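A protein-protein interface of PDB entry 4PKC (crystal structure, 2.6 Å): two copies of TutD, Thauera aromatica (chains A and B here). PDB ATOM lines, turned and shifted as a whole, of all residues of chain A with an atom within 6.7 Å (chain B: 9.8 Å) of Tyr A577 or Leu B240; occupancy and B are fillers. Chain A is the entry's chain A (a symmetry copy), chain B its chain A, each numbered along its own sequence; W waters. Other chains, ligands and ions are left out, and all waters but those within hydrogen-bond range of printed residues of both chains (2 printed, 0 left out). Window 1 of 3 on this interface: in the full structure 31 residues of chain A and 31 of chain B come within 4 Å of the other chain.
The side-chain carboxylate (OD2) of Asp A573 lies within hydrogen-bond range of the indole nitrogen (NE1) of Trp B234. The side-chain hydroxyl (OH) of Tyr A172 is in hydrogen-bond range of the side-chain carboxylate (OD1) of Asp B247 (2.6 Å).
The backbone carbonyl oxygen of Tyr A577 lies within hydrogen-bond range of the guanidinium group of Arg A581. N of Tyr A696 is in hydrogen-bond range of OD1 of Asp A573 (3.0 Å).
Among the printed residues, merely in contact across the chains: Tyr A172 with Pro B89 (3.6 Å), Tyr A172 with Ile B243 (3.7 Å), Ser A570 with Trp B234 (3.7 Å), Asp A573 with Gly B236 (3.5 Å), Asp A573 with Leu B240 (3.5 Å), Val A574 with Leu B240 (3.9 Å), Tyr A577 with Leu B240 (3.8 Å) and Tyr A577 with Ile B243 (3.6 Å).
Tyr A577 touches two residues of chain B. Leu B240 touches just these residues of chain A: Asp A573 (3.5 Å), Val A574 (3.9 Å) and Tyr A577 (3.8 Å). Phe A578 touches none of the printed residues of chain B. Printed residues of chain B within 4 Å of Tyr A172: Pro B89 (3.6 Å), Ile B243 (3.7 Å) and Asp B247 (2.6 Å). Of the printed residues of chain A, Trp B234 touches Ser A570 and Asp A573. Of the printed residues of chain A, Gly B236 touches Asp A573 (3.5 Å). Printed residues of chain B within 4 Å of Asp A573: Trp B234, Gly B236 and Leu B240. Printed residues of chain A within 4 Å of Ile B243: Tyr A172 and Tyr A577. Ala B244 touches none of the printed residues of chain A.
Of the 16 printed residues of chain A, 5 touch a printed residue of chain B. Printed residues of chain A that touch a printed residue of chain B: Tyr A172, Ser A570, Asp A573, Val A574 and Tyr A577.
No position is printed for both chains. Of the 10 pairs that touch across the chains among the printed residues, none has its exchanged pair printed and touching as well.
Water W1 bridges OH of Tyr A172 (2.6 Å) and OD2 of Asp B247 (2.8 Å). Water W2 lies within hydrogen-bond range of O of Leu B240 (2.8 Å), N of Ala B244 (2.8 Å) and OH of Tyr A577 (3.0 Å).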
ATOM      1  N   LEU A 165     -25.165   1.426 -18.796  1.00  0.00           N
ATOM      2  CA  LEU A 165     -25.843   2.698 -18.581  1.00  0.00           C
ATOM      3  C   LEU A 165     -25.455   3.296 -17.235  1.00  0.00           C
ATOM      4  O   LEU A 165     -25.353   4.513 -17.087  1.00  0.00           O
ATOM      5  CB  LEU A 165     -27.358   2.513 -18.662  1.00  0.00           C
ATOM      6  CG  LEU A 165     -28.221   3.752 -18.417  1.00  0.00           C
ATOM      7  CD1 LEU A 165     -27.945   4.816 -19.472  1.00  0.00           C
ATOM      8  CD2 LEU A 165     -29.697   3.379 -18.389  1.00  0.00           C
ATOM      9  N   TYR A 172     -21.173  12.038 -13.612  1.00  0.00           N
ATOM     10  CA  TYR A 172     -21.746  13.378 -13.587  1.00  0.00           C
ATOM     11  C   TYR A 172     -22.562  13.615 -12.322  1.00  0.00           C
ATOM     12  O   TYR A 172     -23.482  14.434 -12.303  1.00  0.00           O
ATOM     13  CB  TYR A 172     -22.601  13.605 -14.834  1.00  0.00           C
ATOM     14  CG  TYR A 172     -21.861  13.273 -16.108  1.00  0.00           C
ATOM     15  CD1 TYR A 172     -21.037  14.208 -16.721  1.00  0.00           C
ATOM     16  CD2 TYR A 172     -21.970  12.015 -16.687  1.00  0.00           C
ATOM     17  CE1 TYR A 172     -20.351  13.903 -17.882  1.00  0.00           C
ATOM     18  CE2 TYR A 172     -21.287  11.702 -17.844  1.00  0.00           C
ATOM     19  CZ  TYR A 172     -20.481  12.648 -18.439  1.00  0.00           C
ATOM     20  OH  TYR A 172     -19.804  12.332 -19.594  1.00  0.00           O
ATOM     21  N   SER A 508     -37.345   6.970 -17.410  1.00  0.00           N
ATOM     22  CA  SER A 508     -36.619   8.227 -17.259  1.00  0.00           C
ATOM     23  C   SER A 508     -37.547   9.428 -17.418  1.00  0.00           C
ATOM     24  O   SER A 508     -37.343  10.470 -16.793  1.00  0.00           O
ATOM     25  CB  SER A 508     -35.478   8.312 -18.275  1.00  0.00           C
ATOM     26  OG  SER A 508     -34.526   7.285 -18.065  1.00  0.00           O
ATOM     27  N   SER A 570     -32.763  14.940 -11.865  1.00  0.00           N
ATOM     28  CA  SER A 570     -31.527  15.119 -12.617  1.00  0.00           C
ATOM     29  C   SER A 570     -30.947  13.775 -13.040  1.00  0.00           C
ATOM     30  O   SER A 570     -30.433  13.636 -14.149  1.00  0.00           O
ATOM     31  CB  SER A 570     -30.498  15.899 -11.796  1.00  0.00           C
ATOM     32  OG  SER A 570     -30.161  15.204 -10.608  1.00  0.00           O
ATOM     33  N   LYS A 572     -32.584  11.107 -13.671  1.00  0.00           N
ATOM     34  CA  LYS A 572     -33.422  10.524 -14.710  1.00  0.00           C
ATOM     35  C   LYS A 572     -33.143  11.173 -16.061  1.00  0.00           C
ATOM     36  O   LYS A 572     -33.142  10.501 -17.093  1.00  0.00           O
ATOM     37  CB  LYS A 572     -34.903  10.658 -14.351  1.00  0.00           C
ATOM     38  CG  LYS A 572     -35.324   9.829 -13.146  1.00  0.00           C
ATOM     39  CD  LYS A 572     -36.835   9.828 -12.968  1.00  0.00           C
ATOM     40  CE  LYS A 572     -37.364  11.225 -12.690  1.00  0.00           C
ATOM     41  NZ  LYS A 572     -38.848  11.239 -12.555  1.00  0.00           N
ATOM     42  N   ASP A 573     -32.900  12.479 -16.050  1.00  0.00           N
ATOM     43  CA  ASP A 573     -32.604  13.208 -17.278  1.00  0.00           C
ATOM     44  C   ASP A 573     -31.219  12.857 -17.809  1.00  0.00           C
ATOM     45  O   ASP A 573     -31.019  12.749 -19.019  1.00  0.00           O
ATOM     46  CB  ASP A 573     -32.719  14.716 -17.050  1.00  0.00           C
ATOM     47  CG  ASP A 573     -34.158  15.180 -16.955  1.00  0.00           C
ATOM     48  OD1 ASP A 573     -35.033  14.531 -17.565  1.00  0.00           O
ATOM     49  OD2 ASP A 573     -34.414  16.196 -16.274  1.00  0.00           O
ATOM     50  N   VAL A 574     -30.263  12.683 -16.902  1.00  0.00           N
ATOM     51  CA  VAL A 574     -28.921  12.258 -17.282  1.00  0.00           C
ATOM     52  C   VAL A 574     -28.981  10.864 -17.898  1.00  0.00           C
ATOM     53  O   VAL A 574     -28.318  10.584 -18.898  1.00  0.00           O
ATOM     54  CB  VAL A 574     -27.959  12.267 -16.075  1.00  0.00           C
ATOM     55  CG1 VAL A 574     -26.700  11.464 -16.374  1.00  0.00           C
ATOM     56  CG2 VAL A 574     -27.607  13.696 -15.696  1.00  0.00           C
ATOM     57  N   SER A 575     -29.795   9.999 -17.301  1.00  0.00           N
ATOM     58  CA  SER A 575     -30.029   8.668 -17.842  1.00  0.00           C
ATOM     59  C   SER A 575     -30.624   8.765 -19.241  1.00  0.00           C
ATOM     60  O   SER A 575     -30.194   8.066 -20.157  1.00  0.00           O
ATOM     61  CB  SER A 575     -30.954   7.867 -16.926  1.00  0.00           C
ATOM     62  OG  SER A 575     -31.208   6.579 -17.456  1.00  0.00           O
ATOM     63  N   ARG A 576     -31.607   9.646 -19.395  1.00  0.00           N
ATOM     64  CA  ARG A 576     -32.253   9.880 -20.683  1.00  0.00           C
ATOM     65  C   ARG A 576     -31.242  10.312 -21.738  1.00  0.00           C
ATOM     66  O   ARG A 576     -31.361   9.959 -22.913  1.00  0.00           O
ATOM     67  CB  ARG A 576     -33.344  10.943 -20.543  1.00  0.00           C
ATOM     68  CG  ARG A 576     -34.208  11.129 -21.778  1.00  0.00           C
ATOM     69  CD  ARG A 576     -35.117   9.933 -21.994  1.00  0.00           C
ATOM     70  NE  ARG A 576     -36.236  10.245 -22.879  1.00  0.00           N
ATOM     71  CZ  ARG A 576     -37.360  10.834 -22.481  1.00  0.00           C
ATOM     72  NH1 ARG A 576     -37.513  11.183 -21.210  1.00  0.00           N
ATOM     73  NH2 ARG A 576     -38.330  11.078 -23.351  1.00  0.00           N
ATOM     74  N   TYR A 577     -30.246  11.078 -21.303  1.00  0.00           N
ATOM     75  CA  TYR A 577     -29.203  11.586 -22.184  1.00  0.00           C
ATOM     76  C   TYR A 577     -28.406  10.446 -22.813  1.00  0.00           C
ATOM     77  O   TYR A 577     -28.112  10.470 -24.007  1.00  0.00           O
ATOM     78  CB  TYR A 577     -28.273  12.525 -21.408  1.00  0.00           C
ATOM     79  CG  TYR A 577     -27.198  13.192 -22.239  1.00  0.00           C
ATOM     80  CD1 TYR A 577     -25.972  12.573 -22.453  1.00  0.00           C
ATOM     81  CD2 TYR A 577     -27.400  14.451 -22.791  1.00  0.00           C
ATOM     82  CE1 TYR A 577     -24.983  13.180 -23.203  1.00  0.00           C
ATOM     83  CE2 TYR A 577     -26.416  15.068 -23.543  1.00  0.00           C
ATOM     84  CZ  TYR A 577     -25.210  14.427 -23.746  1.00  0.00           C
ATOM     85  OH  TYR A 577     -24.226  15.035 -24.493  1.00  0.00           O
ATOM     86  N   PHE A 578     -28.066   9.446 -22.007  1.00  0.00           N
ATOM     87  CA  PHE A 578     -27.238   8.340 -22.476  1.00  0.00           C
ATOM     88  C   PHE A 578     -28.063   7.177 -23.016  1.00  0.00           C
ATOM     89  O   PHE A 578     -27.542   6.327 -23.740  1.00  0.00           O
ATOM     90  CB  PHE A 578     -26.319   7.856 -21.354  1.00  0.00           C
ATOM     91  CG  PHE A 578     -25.258   8.848 -20.980  1.00  0.00           C
ATOM     92  CD1 PHE A 578     -24.151   9.031 -21.793  1.00  0.00           C
ATOM     93  CD2 PHE A 578     -25.369   9.604 -19.825  1.00  0.00           C
ATOM     94  CE1 PHE A 578     -23.174   9.945 -21.459  1.00  0.00           C
ATOM     95  CE2 PHE A 578     -24.392  10.521 -19.486  1.00  0.00           C
ATOM     96  CZ  PHE A 578     -23.293  10.690 -20.306  1.00  0.00           C
ATOM     97  N   GLU A 579     -29.345   7.139 -22.667  1.00  0.00           N
ATOM     98  CA  GLU A 579     -30.237   6.109 -23.186  1.00  0.00           C
ATOM     99  C   GLU A 579     -30.432   6.267 -24.687  1.00  0.00           C
ATOM    100  O   GLU A 579     -30.438   5.288 -25.425  1.00  0.00           O
ATOM    101  CB  GLU A 579     -31.591   6.150 -22.478  1.00  0.00           C
ATOM    102  CG  GLU A 579     -31.609   5.471 -21.121  1.00  0.00           C
ATOM    103  CD  GLU A 579     -32.958   5.581 -20.439  1.00  0.00           C
ATOM    104  OE1 GLU A 579     -33.926   4.959 -20.928  1.00  0.00           O
ATOM    105  OE2 GLU A 579     -33.051   6.298 -19.420  1.00  0.00           O
ATOM    106  N   GLN A 580     -30.584   7.507 -25.140  1.00  0.00           N
ATOM    107  CA  GLN A 580     -30.802   7.771 -26.557  1.00  0.00           C
ATOM    108  C   GLN A 580     -29.505   7.705 -27.357  1.00  0.00           C
ATOM    109  O   GLN A 580     -29.528   7.659 -28.586  1.00  0.00           O
ATOM    110  CB  GLN A 580     -31.459   9.138 -26.747  1.00  0.00           C
ATOM    111  CG  GLN A 580     -30.696  10.286 -26.112  1.00  0.00           C
ATOM    112  CD  GLN A 580     -31.385  11.620 -26.318  1.00  0.00           C
ATOM    113  OE1 GLN A 580     -31.367  12.178 -27.416  1.00  0.00           O
ATOM    114  NE2 GLN A 580     -32.005  12.136 -25.262  1.00  0.00           N
ATOM    115  N   ARG A 581     -28.378   7.692 -26.656  1.00  0.00           N
ATOM    116  CA  ARG A 581     -27.079   7.727 -27.316  1.00  0.00           C
ATOM    117  C   ARG A 581     -26.401   6.360 -27.371  1.00  0.00           C
ATOM    118  O   ARG A 581     -25.627   6.088 -28.289  1.00  0.00           O
ATOM    119  CB  ARG A 581     -26.166   8.737 -26.620  1.00  0.00           C
ATOM    120  CG  ARG A 581     -26.503  10.181 -26.954  1.00  0.00           C
ATOM    121  CD  ARG A 581     -25.775  11.161 -26.052  1.00  0.00           C
ATOM    122  NE  ARG A 581     -25.966  12.537 -26.493  1.00  0.00           N
ATOM    123  CZ  ARG A 581     -27.070  13.247 -26.277  1.00  0.00           C
ATOM    124  NH1 ARG A 581     -28.091  12.710 -25.624  1.00  0.00           N
ATOM    125  NH2 ARG A 581     -27.153  14.495 -26.719  1.00  0.00           N
ATOM    126  N   PHE A 582     -26.693   5.501 -26.400  1.00  0.00           N
ATOM    127  CA  PHE A 582     -26.041   4.196 -26.332  1.00  0.00           C
ATOM    128  C   PHE A 582     -27.020   3.042 -26.123  1.00  0.00           C
ATOM    129  O   PHE A 582     -26.680   1.886 -26.365  1.00  0.00           O
ATOM    130  CB  PHE A 582     -24.992   4.192 -25.219  1.00  0.00           C
ATOM    131  CG  PHE A 582     -23.833   5.113 -25.476  1.00  0.00           C
ATOM    132  CD1 PHE A 582     -22.758   4.696 -26.243  1.00  0.00           C
ATOM    133  CD2 PHE A 582     -23.818   6.395 -24.952  1.00  0.00           C
ATOM    134  CE1 PHE A 582     -21.689   5.541 -26.483  1.00  0.00           C
ATOM    135  CE2 PHE A 582     -22.752   7.243 -25.188  1.00  0.00           C
ATOM    136  CZ  PHE A 582     -21.687   6.816 -25.954  1.00  0.00           C
ATOM    137  N   TYR A 696     -36.626  16.492 -19.149  1.00  0.00           N
ATOM    138  CA  TYR A 696     -36.110  16.400 -20.513  1.00  0.00           C
ATOM    139  C   TYR A 696     -37.122  16.822 -21.578  1.00  0.00           C
ATOM    140  O   TYR A 696     -36.747  17.366 -22.616  1.00  0.00           O
ATOM    141  CB  TYR A 696     -35.636  14.967 -20.782  1.00  0.00           C
ATOM    142  CG  TYR A 696     -35.255  14.687 -22.219  1.00  0.00           C
ATOM    143  CD1 TYR A 696     -33.987  14.997 -22.694  1.00  0.00           C
ATOM    144  CD2 TYR A 696     -36.156  14.094 -23.096  1.00  0.00           C
ATOM    145  CE1 TYR A 696     -33.631  14.735 -24.004  1.00  0.00           C
ATOM    146  CE2 TYR A 696     -35.811  13.830 -24.407  1.00  0.00           C
ATOM    147  CZ  TYR A 696     -34.547  14.152 -24.856  1.00  0.00           C
ATOM    148  OH  TYR A 696     -34.199  13.890 -26.160  1.00  0.00           O
ATOM    149  N   PRO B  89     -16.287   8.853 -22.526  1.00  0.00           N
ATOM    150  CA  PRO B  89     -16.586   9.833 -23.578  1.00  0.00           C
ATOM    151  C   PRO B  89     -15.441   9.936 -24.581  1.00  0.00           C
ATOM    152  O   PRO B  89     -14.281   9.949 -24.170  1.00  0.00           O
ATOM    153  CB  PRO B  89     -16.760  11.142 -22.803  1.00  0.00           C
ATOM    154  CG  PRO B  89     -17.156  10.720 -21.432  1.00  0.00           C
ATOM    155  CD  PRO B  89     -16.419   9.436 -21.178  1.00  0.00           C
ATOM    156  N   ALA B 225     -19.623  24.060 -13.886  1.00  0.00           N
ATOM    157  CA  ALA B 225     -20.602  23.250 -14.602  1.00  0.00           C
ATOM    158  C   ALA B 225     -21.245  22.222 -13.676  1.00  0.00           C
ATOM    159  O   ALA B 225     -22.445  21.962 -13.762  1.00  0.00           O
ATOM    160  CB  ALA B 225     -19.950  22.559 -15.789  1.00  0.00           C
ATOM    161  N   ASP B 228     -23.655  23.928 -11.438  1.00  0.00           N
ATOM    162  CA  ASP B 228     -24.883  24.248 -12.155  1.00  0.00           C
ATOM    163  C   ASP B 228     -25.815  23.043 -12.239  1.00  0.00           C
ATOM    164  O   ASP B 228     -27.034  23.186 -12.146  1.00  0.00           O
ATOM    165  CB  ASP B 228     -24.568  24.757 -13.562  1.00  0.00           C
ATOM    166  CG  ASP B 228     -25.814  25.182 -14.317  1.00  0.00           C
ATOM    167  OD1 ASP B 228     -26.605  25.973 -13.761  1.00  0.00           O
ATOM    168  OD2 ASP B 228     -26.009  24.717 -15.460  1.00  0.00           O
ATOM    169  N   MET B 229     -25.239  21.858 -12.418  1.00  0.00           N
ATOM    170  CA  MET B 229     -26.035  20.641 -12.551  1.00  0.00           C
ATOM    171  C   MET B 229     -26.690  20.247 -11.232  1.00  0.00           C
ATOM    172  O   MET B 229     -27.704  19.550 -11.219  1.00  0.00           O
ATOM    173  CB  MET B 229     -25.175  19.490 -13.077  1.00  0.00           C
ATOM    174  CG  MET B 229     -24.773  19.637 -14.536  1.00  0.00           C
ATOM    175  SD  MET B 229     -23.955  18.169 -15.190  1.00  0.00           S
ATOM    176  CE  MET B 229     -25.259  16.951 -15.027  1.00  0.00           C
ATOM    177  N   SER B 230     -26.110  20.697 -10.125  1.00  0.00           N
ATOM    178  CA  SER B 230     -26.668  20.417  -8.807  1.00  0.00           C
ATOM    179  C   SER B 230     -27.389  21.639  -8.248  1.00  0.00           C
ATOM    180  O   SER B 230     -27.633  21.731  -7.045  1.00  0.00           O
ATOM    181  CB  SER B 230     -25.571  19.968  -7.841  1.00  0.00           C
ATOM    182  OG  SER B 230     -24.637  21.010  -7.618  1.00  0.00           O
ATOM    183  N   TRP B 234     -33.661  22.103 -11.055  1.00  0.00           N
ATOM    184  CA  TRP B 234     -33.081  21.478 -12.238  1.00  0.00           C
ATOM    185  C   TRP B 234     -33.926  21.743 -13.482  1.00  0.00           C
ATOM    186  O   TRP B 234     -35.153  21.791 -13.414  1.00  0.00           O
ATOM    187  CB  TRP B 234     -32.920  19.970 -12.010  1.00  0.00           C
ATOM    188  CG  TRP B 234     -32.601  19.188 -13.250  1.00  0.00           C
ATOM    189  CD1 TRP B 234     -33.491  18.555 -14.070  1.00  0.00           C
ATOM    190  CD2 TRP B 234     -31.303  18.950 -13.809  1.00  0.00           C
ATOM    191  NE1 TRP B 234     -32.827  17.941 -15.103  1.00  0.00           N
ATOM    192  CE2 TRP B 234     -31.484  18.167 -14.967  1.00  0.00           C
ATOM    193  CE3 TRP B 234     -30.005  19.323 -13.443  1.00  0.00           C
ATOM    194  CZ2 TRP B 234     -30.418  17.753 -15.762  1.00  0.00           C
ATOM    195  CZ3 TRP B 234     -28.948  18.909 -14.234  1.00  0.00           C
ATOM    196  CH2 TRP B 234     -29.161  18.132 -15.380  1.00  0.00           C
ATOM    197  N   ASN B 235     -33.256  21.922 -14.615  1.00  0.00           N
ATOM    198  CA  ASN B 235     -33.933  22.116 -15.892  1.00  0.00           C
ATOM    199  C   ASN B 235     -33.346  21.184 -16.945  1.00  0.00           C
ATOM    200  O   ASN B 235     -32.273  21.446 -17.493  1.00  0.00           O
ATOM    201  CB  ASN B 235     -33.820  23.575 -16.345  1.00  0.00           C
ATOM    202  CG  ASN B 235     -34.786  23.921 -17.467  1.00  0.00           C
ATOM    203  OD1 ASN B 235     -35.149  23.072 -18.281  1.00  0.00           O
ATOM    204  ND2 ASN B 235     -35.205  25.179 -17.514  1.00  0.00           N
ATOM    205  N   GLY B 236     -34.062  20.099 -17.228  1.00  0.00           N
ATOM    206  CA  GLY B 236     -33.586  19.064 -18.130  1.00  0.00           C
ATOM    207  C   GLY B 236     -33.402  19.505 -19.568  1.00  0.00           C
ATOM    208  O   GLY B 236     -32.761  18.811 -20.359  1.00  0.00           O
ATOM    209  N   THR B 237     -33.964  20.658 -19.914  1.00  0.00           N
ATOM    210  CA  THR B 237     -33.837  21.186 -21.266  1.00  0.00           C
ATOM    211  C   THR B 237     -32.575  22.025 -21.418  1.00  0.00           C
ATOM    212  O   THR B 237     -32.218  22.429 -22.524  1.00  0.00           O
ATOM    213  CB  THR B 237     -35.057  22.039 -21.656  1.00  0.00           C
ATOM    214  OG1 THR B 237     -35.149  23.174 -20.785  1.00  0.00           O
ATOM    215  CG2 THR B 237     -36.329  21.219 -21.549  1.00  0.00           C
ATOM    216  N   LYS B 238     -31.899  22.280 -20.300  1.00  0.00           N
ATOM    217  CA  LYS B 238     -30.692  23.099 -20.305  1.00  0.00           C
ATOM    218  C   LYS B 238     -29.531  22.421 -19.586  1.00  0.00           C
ATOM    219  O   LYS B 238     -28.395  22.454 -20.058  1.00  0.00           O
ATOM    220  CB  LYS B 238     -30.964  24.459 -19.658  1.00  0.00           C
ATOM    221  CG  LYS B 238     -31.977  25.319 -20.391  1.00  0.00           C
ATOM    222  CD  LYS B 238     -32.144  26.665 -19.703  1.00  0.00           C
ATOM    223  CE  LYS B 238     -33.103  27.560 -20.466  1.00  0.00           C
ATOM    224  NZ  LYS B 238     -33.229  28.902 -19.830  1.00  0.00           N
ATOM    225  N   GLY B 239     -29.825  21.809 -18.443  1.00  0.00           N
ATOM    226  CA  GLY B 239     -28.801  21.247 -17.580  1.00  0.00           C
ATOM    227  C   GLY B 239     -27.927  20.178 -18.207  1.00  0.00           C
ATOM    228  O   GLY B 239     -26.783  19.984 -17.795  1.00  0.00           O
ATOM    229  N   LEU B 240     -28.458  19.484 -19.209  1.00  0.00           N
ATOM    230  CA  LEU B 240     -27.729  18.394 -19.849  1.00  0.00           C
ATOM    231  C   LEU B 240     -26.651  18.905 -20.802  1.00  0.00           C
ATOM    232  O   LEU B 240     -25.846  18.127 -21.315  1.00  0.00           O
ATOM    233  CB  LEU B 240     -28.697  17.473 -20.598  1.00  0.00           C
ATOM    234  CG  LEU B 240     -29.731  16.755 -19.730  1.00  0.00           C
ATOM    235  CD1 LEU B 240     -30.629  15.865 -20.576  1.00  0.00           C
ATOM    236  CD2 LEU B 240     -29.044  15.950 -18.637  1.00  0.00           C
ATOM    237  N   ASP B 241     -26.635  20.215 -21.030  1.00  0.00           N
ATOM    238  CA  ASP B 241     -25.632  20.829 -21.894  1.00  0.00           C
ATOM    239  C   ASP B 241     -24.249  20.794 -21.252  1.00  0.00           C
ATOM    240  O   ASP B 241     -23.234  20.874 -21.942  1.00  0.00           O
ATOM    241  CB  ASP B 241     -26.017  22.274 -22.223  1.00  0.00           C
ATOM    242  CG  ASP B 241     -27.202  22.362 -23.165  1.00  0.00           C
ATOM    243  OD1 ASP B 241     -27.940  21.363 -23.292  1.00  0.00           O
ATOM    244  OD2 ASP B 241     -27.395  23.433 -23.777  1.00  0.00           O
ATOM    245  N   ASN B 242     -24.218  20.676 -19.929  1.00  0.00           N
ATOM    246  CA  ASN B 242     -22.963  20.667 -19.189  1.00  0.00           C
ATOM    247  C   ASN B 242     -22.164  19.383 -19.399  1.00  0.00           C
ATOM    248  O   ASN B 242     -20.955  19.355 -19.171  1.00  0.00           O
ATOM    249  CB  ASN B 242     -23.223  20.873 -17.695  1.00  0.00           C
ATOM    250  CG  ASN B 242     -23.770  22.252 -17.381  1.00  0.00           C
ATOM    251  OD1 ASN B 242     -23.016  23.217 -17.244  1.00  0.00           O
ATOM    252  ND2 ASN B 242     -25.089  22.352 -17.259  1.00  0.00           N
ATOM    253  N   ILE B 243     -22.842  18.327 -19.835  1.00  0.00           N
ATOM    254  CA  ILE B 243     -22.199  17.030 -20.024  1.00  0.00           C
ATOM    255  C   ILE B 243     -21.085  17.091 -21.067  1.00  0.00           C
ATOM    256  O   ILE B 243     -19.954  16.686 -20.796  1.00  0.00           O
ATOM    257  CB  ILE B 243     -23.221  15.951 -20.434  1.00  0.00           C
ATOM    258  CG1 ILE B 243     -24.238  15.732 -19.312  1.00  0.00           C
ATOM    259  CG2 ILE B 243     -22.514  14.647 -20.767  1.00  0.00           C
ATOM    260  CD1 ILE B 243     -25.287  14.691 -19.628  1.00  0.00           C
ATOM    261  N   ALA B 244     -21.402  17.605 -22.252  1.00  0.00           N
ATOM    262  CA  ALA B 244     -20.416  17.714 -23.324  1.00  0.00           C
ATOM    263  C   ALA B 244     -19.285  18.662 -22.942  1.00  0.00           C
ATOM    264  O   ALA B 244     -18.135  18.451 -23.323  1.00  0.00           O
ATOM    265  CB  ALA B 244     -21.077  18.174 -24.612  1.00  0.00           C
ATOM    266  N   LYS B 245     -19.620  19.705 -22.190  1.00  0.00           N
ATOM    267  CA  LYS B 245     -18.628  20.687 -21.763  1.00  0.00           C
ATOM    268  C   LYS B 245     -17.640  20.082 -20.771  1.00  0.00           C
ATOM    269  O   LYS B 245     -16.426  20.225 -20.930  1.00  0.00           O
ATOM    270  CB  LYS B 245     -19.313  21.907 -21.144  1.00  0.00           C
ATOM    271  CG  LYS B 245     -20.185  22.690 -22.110  1.00  0.00           C
ATOM    272  CD  LYS B 245     -20.855  23.864 -21.415  1.00  0.00           C
ATOM    273  CE  LYS B 245     -21.805  24.594 -22.349  1.00  0.00           C
ATOM    274  NZ  LYS B 245     -22.511  25.701 -21.651  1.00  0.00           N
ATOM    275  N   ILE B 246     -18.166  19.411 -19.751  1.00  0.00           N
ATOM    276  CA  ILE B 246     -17.337  18.772 -18.733  1.00  0.00           C
ATOM    277  C   ILE B 246     -16.416  17.725 -19.355  1.00  0.00           C
ATOM    278  O   ILE B 246     -15.238  17.632 -19.003  1.00  0.00           O
ATOM    279  CB  ILE B 246     -18.200  18.114 -17.635  1.00  0.00           C
ATOM    280  CG1 ILE B 246     -18.924  19.185 -16.819  1.00  0.00           C
ATOM    281  CG2 ILE B 246     -17.346  17.264 -16.712  1.00  0.00           C
ATOM    282  CD1 ILE B 246     -19.872  18.624 -15.786  1.00  0.00           C
ATOM    283  N   ASP B 247     -16.956  16.948 -20.289  1.00  0.00           N
ATOM    284  CA  ASP B 247     -16.173  15.943 -20.998  1.00  0.00           C
ATOM    285  C   ASP B 247     -15.022  16.580 -21.771  1.00  0.00           C
ATOM    286  O   ASP B 247     -13.899  16.074 -21.762  1.00  0.00           O
ATOM    287  CB  ASP B 247     -17.061  15.139 -21.948  1.00  0.00           C
ATOM    288  CG  ASP B 247     -18.031  14.233 -21.214  1.00  0.00           C
ATOM    289  OD1 ASP B 247     -17.729  13.844 -20.067  1.00  0.00           O
ATOM    290  OD2 ASP B 247     -19.093  13.907 -21.786  1.00  0.00           O
ATOM    291  N   ASN B 248     -15.306  17.696 -22.436  1.00  0.00           N
ATOM    292  CA  ASN B 248     -14.293  18.404 -23.206  1.00  0.00           C
ATOM    293  C   ASN B 248     -13.224  19.028 -22.315  1.00  0.00           C
ATOM    294  O   ASN B 248     -12.031  18.903 -22.589  1.00  0.00           O
ATOM    295  CB  ASN B 248     -14.941  19.480 -24.077  1.00  0.00           C
ATOM    296  CG  ASN B 248     -15.523  18.919 -25.361  1.00  0.00           C
ATOM    297  OD1 ASN B 248     -14.952  18.014 -25.969  1.00  0.00           O
ATOM    298  ND2 ASN B 248     -16.661  19.458 -25.781  1.00  0.00           N
HETATM  299  O   HOH W   1     -20.485  11.532 -21.925  1.00  0.00           O
HETATM  300  O   HOH W   2     -23.995  17.761 -23.355  1.00  0.00           O
